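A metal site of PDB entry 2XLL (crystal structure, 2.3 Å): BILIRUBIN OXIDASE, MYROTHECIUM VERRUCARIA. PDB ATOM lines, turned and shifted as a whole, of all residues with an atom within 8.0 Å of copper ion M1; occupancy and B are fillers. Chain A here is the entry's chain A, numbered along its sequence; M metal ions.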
ATOM      1  N   HIS A  94      14.224  17.714 -25.060  1.00  0.00           N
ATOM      2  CA  HIS A  94      13.438  17.777 -26.268  1.00  0.00           C
ATOM      3  C   HIS A  94      12.089  18.385 -25.980  1.00  0.00           C
ATOM      4  O   HIS A  94      11.352  17.877 -25.149  1.00  0.00           O
ATOM      5  CB  HIS A  94      13.190  16.388 -26.852  1.00  0.00           C
ATOM      6  CG  HIS A  94      12.258  16.402 -28.015  1.00  0.00           C
ATOM      7  ND1 HIS A  94      12.362  17.311 -29.038  1.00  0.00           N
ATOM      8  CD2 HIS A  94      11.169  15.649 -28.286  1.00  0.00           C
ATOM      9  CE1 HIS A  94      11.397  17.107 -29.911  1.00  0.00           C
ATOM     10  NE2 HIS A  94      10.655  16.104 -29.476  1.00  0.00           N
ATOM     11  N   LEU A  95      11.775  19.459 -26.692  1.00  0.00           N
ATOM     12  CA  LEU A  95      10.456  20.059 -26.608  1.00  0.00           C
ATOM     13  C   LEU A  95       9.608  19.430 -27.720  1.00  0.00           C
ATOM     14  O   LEU A  95       9.719  19.803 -28.893  1.00  0.00           O
ATOM     15  CB  LEU A  95      10.522  21.575 -26.751  1.00  0.00           C
ATOM     16  CG  LEU A  95       9.149  22.285 -26.756  1.00  0.00           C
ATOM     17  CD1 LEU A  95       8.507  22.215 -25.385  1.00  0.00           C
ATOM     18  CD2 LEU A  95       9.256  23.736 -27.211  1.00  0.00           C
ATOM     19  N   HIS A  96       8.778  18.473 -27.330  1.00  0.00           N
ATOM     20  CA  HIS A  96       7.986  17.677 -28.246  1.00  0.00           C
ATOM     21  C   HIS A  96       6.745  18.425 -28.735  1.00  0.00           C
ATOM     22  O   HIS A  96       5.906  18.831 -27.938  1.00  0.00           O
ATOM     23  CB  HIS A  96       7.544  16.415 -27.507  1.00  0.00           C
ATOM     24  CG  HIS A  96       6.798  15.434 -28.347  1.00  0.00           C
ATOM     25  ND1 HIS A  96       7.077  14.085 -28.325  1.00  0.00           N
ATOM     26  CD2 HIS A  96       5.773  15.598 -29.222  1.00  0.00           C
ATOM     27  CE1 HIS A  96       6.262  13.457 -29.153  1.00  0.00           C
ATOM     28  NE2 HIS A  96       5.459  14.349 -29.710  1.00  0.00           N
ATOM     29  N   GLY A  97       6.620  18.568 -30.055  1.00  0.00           N
ATOM     30  CA  GLY A  97       5.522  19.331 -30.633  1.00  0.00           C
ATOM     31  C   GLY A  97       5.956  20.672 -31.208  1.00  0.00           C
ATOM     32  O   GLY A  97       5.119  21.400 -31.714  1.00  0.00           O
ATOM     33  N   TRP A 132       5.097  19.272 -24.621  1.00  0.00           N
ATOM     34  CA  TRP A 132       5.729  18.836 -23.386  1.00  0.00           C
ATOM     35  C   TRP A 132       7.209  18.682 -23.618  1.00  0.00           C
ATOM     36  O   TRP A 132       7.628  18.304 -24.689  1.00  0.00           O
ATOM     37  CB  TRP A 132       5.077  17.549 -22.847  1.00  0.00           C
ATOM     38  CG  TRP A 132       5.238  16.315 -23.684  1.00  0.00           C
ATOM     39  CD1 TRP A 132       4.879  16.146 -24.989  1.00  0.00           C
ATOM     40  CD2 TRP A 132       5.755  15.047 -23.238  1.00  0.00           C
ATOM     41  NE1 TRP A 132       5.154  14.852 -25.396  1.00  0.00           N
ATOM     42  CE2 TRP A 132       5.700  14.167 -24.336  1.00  0.00           C
ATOM     43  CE3 TRP A 132       6.253  14.580 -22.019  1.00  0.00           C
ATOM     44  CZ2 TRP A 132       6.127  12.844 -24.251  1.00  0.00           C
ATOM     45  CZ3 TRP A 132       6.676  13.266 -21.931  1.00  0.00           C
ATOM     46  CH2 TRP A 132       6.611  12.419 -23.045  1.00  0.00           C
ATOM     47  N   TYR A 133       7.998  19.022 -22.607  1.00  0.00           N
ATOM     48  CA  TYR A 133       9.425  18.874 -22.713  1.00  0.00           C
ATOM     49  C   TYR A 133       9.906  17.706 -21.855  1.00  0.00           C
ATOM     50  O   TYR A 133       9.401  17.476 -20.760  1.00  0.00           O
ATOM     51  CB  TYR A 133      10.115  20.189 -22.324  1.00  0.00           C
ATOM     52  CG  TYR A 133       9.888  20.627 -20.897  1.00  0.00           C
ATOM     53  CD1 TYR A 133       8.698  21.236 -20.519  1.00  0.00           C
ATOM     54  CD2 TYR A 133      10.872  20.437 -19.926  1.00  0.00           C
ATOM     55  CE1 TYR A 133       8.502  21.646 -19.209  1.00  0.00           C
ATOM     56  CE2 TYR A 133      10.684  20.850 -18.620  1.00  0.00           C
ATOM     57  CZ  TYR A 133       9.484  21.452 -18.271  1.00  0.00           C
ATOM     58  OH  TYR A 133       9.283  21.854 -16.981  1.00  0.00           O
ATOM     59  N   HIS A 134      10.906  16.982 -22.349  1.00  0.00           N
ATOM     60  CA  HIS A 134      11.381  15.804 -21.644  1.00  0.00           C
ATOM     61  C   HIS A 134      12.713  15.355 -22.180  1.00  0.00           C
ATOM     62  O   HIS A 134      13.128  15.746 -23.264  1.00  0.00           O
ATOM     63  CB  HIS A 134      10.380  14.689 -21.815  1.00  0.00           C
ATOM     64  CG  HIS A 134      10.313  14.167 -23.217  1.00  0.00           C
ATOM     65  ND1 HIS A 134      11.335  13.448 -23.789  1.00  0.00           N
ATOM     66  CD2 HIS A 134       9.327  14.240 -24.150  1.00  0.00           C
ATOM     67  CE1 HIS A 134      10.990  13.106 -25.024  1.00  0.00           C
ATOM     68  NE2 HIS A 134       9.779  13.567 -25.256  1.00  0.00           N
ATOM     69  N   ASP A 135      13.385  14.489 -21.415  1.00  0.00           N
ATOM     70  CA  ASP A 135      14.728  14.053 -21.755  1.00  0.00           C
ATOM     71  C   ASP A 135      14.765  13.149 -22.988  1.00  0.00           C
ATOM     72  O   ASP A 135      13.806  12.433 -23.275  1.00  0.00           O
ATOM     73  CB  ASP A 135      15.370  13.312 -20.590  1.00  0.00           C
ATOM     74  CG  ASP A 135      16.832  13.016 -20.844  1.00  0.00           C
ATOM     75  OD1 ASP A 135      17.614  13.986 -20.934  1.00  0.00           O
ATOM     76  OD2 ASP A 135      17.194  11.816 -20.964  1.00  0.00           O
ATOM     77  N   HIS A 136      15.906  13.153 -23.658  1.00  0.00           N
ATOM     78  CA  HIS A 136      16.069  12.362 -24.866  1.00  0.00           C
ATOM     79  C   HIS A 136      17.504  11.827 -24.968  1.00  0.00           C
ATOM     80  O   HIS A 136      17.926  11.381 -26.023  1.00  0.00           O
ATOM     81  CB  HIS A 136      15.746  13.244 -26.076  1.00  0.00           C
ATOM     82  CG  HIS A 136      14.960  12.563 -27.154  1.00  0.00           C
ATOM     83  ND1 HIS A 136      15.359  11.373 -27.735  1.00  0.00           N
ATOM     84  CD2 HIS A 136      13.805  12.915 -27.766  1.00  0.00           C
ATOM     85  CE1 HIS A 136      14.469  11.018 -28.643  1.00  0.00           C
ATOM     86  NE2 HIS A 136      13.525  11.941 -28.695  1.00  0.00           N
ATOM     87  N   THR A 141      17.112   7.375 -22.096  1.00  0.00           N
ATOM     88  CA  THR A 141      15.896   8.189 -22.125  1.00  0.00           C
ATOM     89  C   THR A 141      14.813   7.595 -21.201  1.00  0.00           C
ATOM     90  O   THR A 141      14.120   8.316 -20.476  1.00  0.00           O
ATOM     91  CB  THR A 141      15.356   8.323 -23.558  1.00  0.00           C
ATOM     92  OG1 THR A 141      16.269   9.105 -24.333  1.00  0.00           O
ATOM     93  CG2 THR A 141      14.009   9.000 -23.566  1.00  0.00           C
ATOM     94  N   LEU A 226      -2.099  13.709 -21.290  1.00  0.00           N
ATOM     95  CA  LEU A 226      -0.817  13.415 -21.913  1.00  0.00           C
ATOM     96  C   LEU A 226      -0.370  12.072 -21.383  1.00  0.00           C
ATOM     97  O   LEU A 226      -0.238  11.900 -20.158  1.00  0.00           O
ATOM     98  CB  LEU A 226       0.222  14.477 -21.553  1.00  0.00           C
ATOM     99  CG  LEU A 226       1.645  13.929 -21.617  1.00  0.00           C
ATOM    100  CD1 LEU A 226       2.065  13.626 -23.061  1.00  0.00           C
ATOM    101  CD2 LEU A 226       2.631  14.864 -20.973  1.00  0.00           C
ATOM    102  N   ASP A 227      -0.178  11.096 -22.262  1.00  0.00           N
ATOM    103  CA  ASP A 227       0.336   9.820 -21.782  1.00  0.00           C
ATOM    104  C   ASP A 227       1.837   9.926 -21.707  1.00  0.00           C
ATOM    105  O   ASP A 227       2.512   9.888 -22.744  1.00  0.00           O
ATOM    106  CB  ASP A 227      -0.055   8.671 -22.682  1.00  0.00           C
ATOM    107  CG  ASP A 227       0.551   7.346 -22.227  1.00  0.00           C
ATOM    108  OD1 ASP A 227       1.205   7.325 -21.164  1.00  0.00           O
ATOM    109  OD2 ASP A 227       0.372   6.335 -22.941  1.00  0.00           O
ATOM    110  N   MET A 273       1.799   6.475 -25.706  1.00  0.00           N
ATOM    111  CA  MET A 273       2.925   7.261 -25.239  1.00  0.00           C
ATOM    112  C   MET A 273       3.208   8.457 -26.162  1.00  0.00           C
ATOM    113  O   MET A 273       3.277   8.327 -27.371  1.00  0.00           O
ATOM    114  CB  MET A 273       4.157   6.368 -25.122  1.00  0.00           C
ATOM    115  CG  MET A 273       4.105   5.295 -24.013  1.00  0.00           C
ATOM    116  SD  MET A 273       3.061   3.841 -24.274  1.00  0.00           S
ATOM    117  CE  MET A 273       3.969   2.957 -25.524  1.00  0.00           C
ATOM    118  N   ALA A 274       3.337   9.623 -25.536  1.00  0.00           N
ATOM    119  CA  ALA A 274       3.655  10.921 -26.147  1.00  0.00           C
ATOM    120  C   ALA A 274       2.450  11.642 -26.744  1.00  0.00           C
ATOM    121  O   ALA A 274       2.545  12.778 -27.170  1.00  0.00           O
ATOM    122  CB  ALA A 274       4.763  10.783 -27.188  1.00  0.00           C
ATOM    123  N   GLU A 275       1.306  10.955 -26.729  1.00  0.00           N
ATOM    124  CA  GLU A 275       0.074  11.502 -27.268  1.00  0.00           C
ATOM    125  C   GLU A 275      -0.636  12.463 -26.342  1.00  0.00           C
ATOM    126  O   GLU A 275      -0.713  12.257 -25.140  1.00  0.00           O
ATOM    127  CB  GLU A 275      -0.893  10.384 -27.655  1.00  0.00           C
ATOM    128  CG  GLU A 275      -0.601   9.741 -28.983  1.00  0.00           C
ATOM    129  CD  GLU A 275      -1.679   8.796 -29.394  1.00  0.00           C
ATOM    130  OE1 GLU A 275      -2.313   8.196 -28.530  1.00  0.00           O
ATOM    131  OE2 GLU A 275      -1.906   8.649 -30.595  1.00  0.00           O
ATOM    132  N   ARG A 276      -1.147  13.525 -26.926  1.00  0.00           N
ATOM    133  CA  ARG A 276      -1.893  14.502 -26.170  1.00  0.00           C
ATOM    134  C   ARG A 276      -3.279  14.705 -26.758  1.00  0.00           C
ATOM    135  O   ARG A 276      -3.428  14.977 -27.924  1.00  0.00           O
ATOM    136  CB  ARG A 276      -1.179  15.850 -26.168  1.00  0.00           C
ATOM    137  CG  ARG A 276       0.151  15.893 -25.459  1.00  0.00           C
ATOM    138  CD  ARG A 276       1.174  16.634 -26.268  1.00  0.00           C
ATOM    139  NE  ARG A 276       1.808  15.747 -27.208  1.00  0.00           N
ATOM    140  CZ  ARG A 276       2.220  16.070 -28.418  1.00  0.00           C
ATOM    141  NH1 ARG A 276       2.079  17.288 -28.892  1.00  0.00           N
ATOM    142  NH2 ARG A 276       2.798  15.140 -29.158  1.00  0.00           N
ATOM    143  N   HIS A 401       6.654   8.415 -33.453  1.00  0.00           N
ATOM    144  CA  HIS A 401       6.822   9.863 -33.383  1.00  0.00           C
ATOM    145  C   HIS A 401       7.806  10.405 -34.419  1.00  0.00           C
ATOM    146  O   HIS A 401       8.907   9.908 -34.569  1.00  0.00           O
ATOM    147  CB  HIS A 401       7.289  10.275 -31.990  1.00  0.00           C
ATOM    148  CG  HIS A 401       7.550  11.731 -31.864  1.00  0.00           C
ATOM    149  ND1 HIS A 401       6.640  12.688 -32.253  1.00  0.00           N
ATOM    150  CD2 HIS A 401       8.644  12.403 -31.423  1.00  0.00           C
ATOM    151  CE1 HIS A 401       7.150  13.884 -32.041  1.00  0.00           C
ATOM    152  NE2 HIS A 401       8.358  13.750 -31.541  1.00  0.00           N
ATOM    153  N   HIS A 403       9.735  13.848 -35.562  1.00  0.00           N
ATOM    154  CA  HIS A 403      10.113  15.187 -35.133  1.00  0.00           C
ATOM    155  C   HIS A 403       9.861  16.217 -36.222  1.00  0.00           C
ATOM    156  O   HIS A 403       9.624  15.859 -37.365  1.00  0.00           O
ATOM    157  CB  HIS A 403      11.584  15.223 -34.748  1.00  0.00           C
ATOM    158  CG  HIS A 403      11.865  14.710 -33.372  1.00  0.00           C
ATOM    159  ND1 HIS A 403      12.665  15.384 -32.478  1.00  0.00           N
ATOM    160  CD2 HIS A 403      11.414  13.608 -32.728  1.00  0.00           C
ATOM    161  CE1 HIS A 403      12.731  14.712 -31.342  1.00  0.00           C
ATOM    162  NE2 HIS A 403      11.972  13.628 -31.472  1.00  0.00           N
ATOM    163  N   ASP A 430       1.398  14.397 -34.024  1.00  0.00           N
ATOM    164  CA  ASP A 430       2.808  14.105 -34.231  1.00  0.00           C
ATOM    165  C   ASP A 430       3.224  12.759 -33.642  1.00  0.00           C
ATOM    166  O   ASP A 430       4.380  12.371 -33.667  1.00  0.00           O
ATOM    167  CB  ASP A 430       3.716  15.258 -33.757  1.00  0.00           C
ATOM    168  CG  ASP A 430       3.563  15.543 -32.265  1.00  0.00           C
ATOM    169  OD1 ASP A 430       3.494  14.572 -31.485  1.00  0.00           O
ATOM    170  OD2 ASP A 430       3.531  16.729 -31.871  1.00  0.00           O
ATOM    171  N   VAL A 431       2.257  12.031 -33.092  1.00  0.00           N
ATOM    172  CA  VAL A 431       2.479  10.654 -32.701  1.00  0.00           C
ATOM    173  C   VAL A 431       1.225   9.864 -33.007  1.00  0.00           C
ATOM    174  O   VAL A 431       0.109  10.352 -32.794  1.00  0.00           O
ATOM    175  CB  VAL A 431       2.892  10.477 -31.222  1.00  0.00           C
ATOM    176  CG1 VAL A 431       2.028  11.328 -30.329  1.00  0.00           C
ATOM    177  CG2 VAL A 431       2.809   8.994 -30.825  1.00  0.00           C
ATOM    178  N   HIS A 456      10.966   7.868 -34.304  1.00  0.00           N
ATOM    179  CA  HIS A 456      11.140   6.667 -33.477  1.00  0.00           C
ATOM    180  C   HIS A 456       9.832   6.217 -32.857  1.00  0.00           C
ATOM    181  O   HIS A 456       8.815   6.909 -32.957  1.00  0.00           O
ATOM    182  CB  HIS A 456      12.144   6.943 -32.341  1.00  0.00           C
ATOM    183  CG  HIS A 456      11.755   8.104 -31.478  1.00  0.00           C
ATOM    184  ND1 HIS A 456      11.100   7.949 -30.273  1.00  0.00           N
ATOM    185  CD2 HIS A 456      11.897   9.438 -31.658  1.00  0.00           C
ATOM    186  CE1 HIS A 456      10.881   9.145 -29.734  1.00  0.00           C
ATOM    187  NE2 HIS A 456      11.357  10.060 -30.557  1.00  0.00           N
ATOM    188  N   HIS A 458       7.758   5.788 -29.423  1.00  0.00           N
ATOM    189  CA  HIS A 458       7.849   6.513 -28.163  1.00  0.00           C
ATOM    190  C   HIS A 458       7.633   5.615 -26.930  1.00  0.00           C
ATOM    191  O   HIS A 458       7.512   6.102 -25.795  1.00  0.00           O
ATOM    192  CB  HIS A 458       6.901   7.723 -28.150  1.00  0.00           C
ATOM    193  CG  HIS A 458       7.487   8.925 -27.474  1.00  0.00           C
ATOM    194  ND1 HIS A 458       7.631   9.004 -26.105  1.00  0.00           N
ATOM    195  CD2 HIS A 458       7.979  10.074 -27.979  1.00  0.00           C
ATOM    196  CE1 HIS A 458       8.177  10.168 -25.790  1.00  0.00           C
ATOM    197  NE2 HIS A 458       8.395  10.835 -26.906  1.00  0.00           N
ATOM    198  N   LEU A 460       9.538   4.172 -24.550  1.00  0.00           N
ATOM    199  CA  LEU A 460      10.909   4.505 -24.198  1.00  0.00           C
ATOM    200  C   LEU A 460      11.840   3.300 -24.113  1.00  0.00           C
ATOM    201  O   LEU A 460      13.021   3.396 -24.418  1.00  0.00           O
ATOM    202  CB  LEU A 460      10.950   5.302 -22.898  1.00  0.00           C
ATOM    203  CG  LEU A 460      10.055   6.542 -22.897  1.00  0.00           C
ATOM    204  CD1 LEU A 460      10.370   7.468 -21.754  1.00  0.00           C
ATOM    205  CD2 LEU A 460      10.207   7.273 -24.200  1.00  0.00           C
ATOM    206  N   GLU A 463      12.546   2.541 -27.658  1.00  0.00           N
ATOM    207  CA  GLU A 463      13.359   3.650 -28.119  1.00  0.00           C
ATOM    208  C   GLU A 463      14.822   3.472 -27.756  1.00  0.00           C
ATOM    209  O   GLU A 463      15.704   3.651 -28.589  1.00  0.00           O
ATOM    210  CB  GLU A 463      12.828   4.961 -27.555  1.00  0.00           C
ATOM    211  CG  GLU A 463      13.404   6.222 -28.182  1.00  0.00           C
ATOM    212  CD  GLU A 463      12.888   7.480 -27.507  1.00  0.00           C
ATOM    213  OE1 GLU A 463      11.654   7.562 -27.298  1.00  0.00           O
ATOM    214  OE2 GLU A 463      13.695   8.357 -27.158  1.00  0.00           O
HETATM  215 CU    CU M   1       8.469  13.103 -26.969  1.00  0.00          CU
HETATM  216 CU    CU M   2       9.249  15.084 -30.424  1.00  0.00          CU
HETATM  217 CU    CU M   3      11.955  12.054 -30.201  1.00  0.00          CU
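Residues that only touch copper ion M1: His 94 and Trp 132. Of the 24 residues printed, 5 come within 4 Å of copper ion M1. The nearest printed residue that does not touch copper ion M1 is Ala 274 (4.4 Å).
ND1 of His 96 is bound to copper ion M1, 2.2 Å away. NE2 of His 134 is bound to copper ion M1 (2.2 Å). Copper ion M1 is bound by a ring nitrogen (NE2) of His 458 (2.3 Å). Copper ion M1 has three donor atoms within binding distance.
NE2 of His 96 lies within hydrogen-bond range of NH2 of Arg 276, 2.8 Å away. NE2 of His 96 sits at hydrogen-bond distance from OD1 of Asp 430 (2.7 Å). O of His 134 is in hydrogen-bond range of N of His 94, at 2.9 Å. A ring nitrogen (ND1) of His 401 sits close to a ring nitrogen (NE2) of His 96 (3.3 Å). N of His 96 is in hydrogen-bond range of O of Trp 132, at 2.9 Å.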
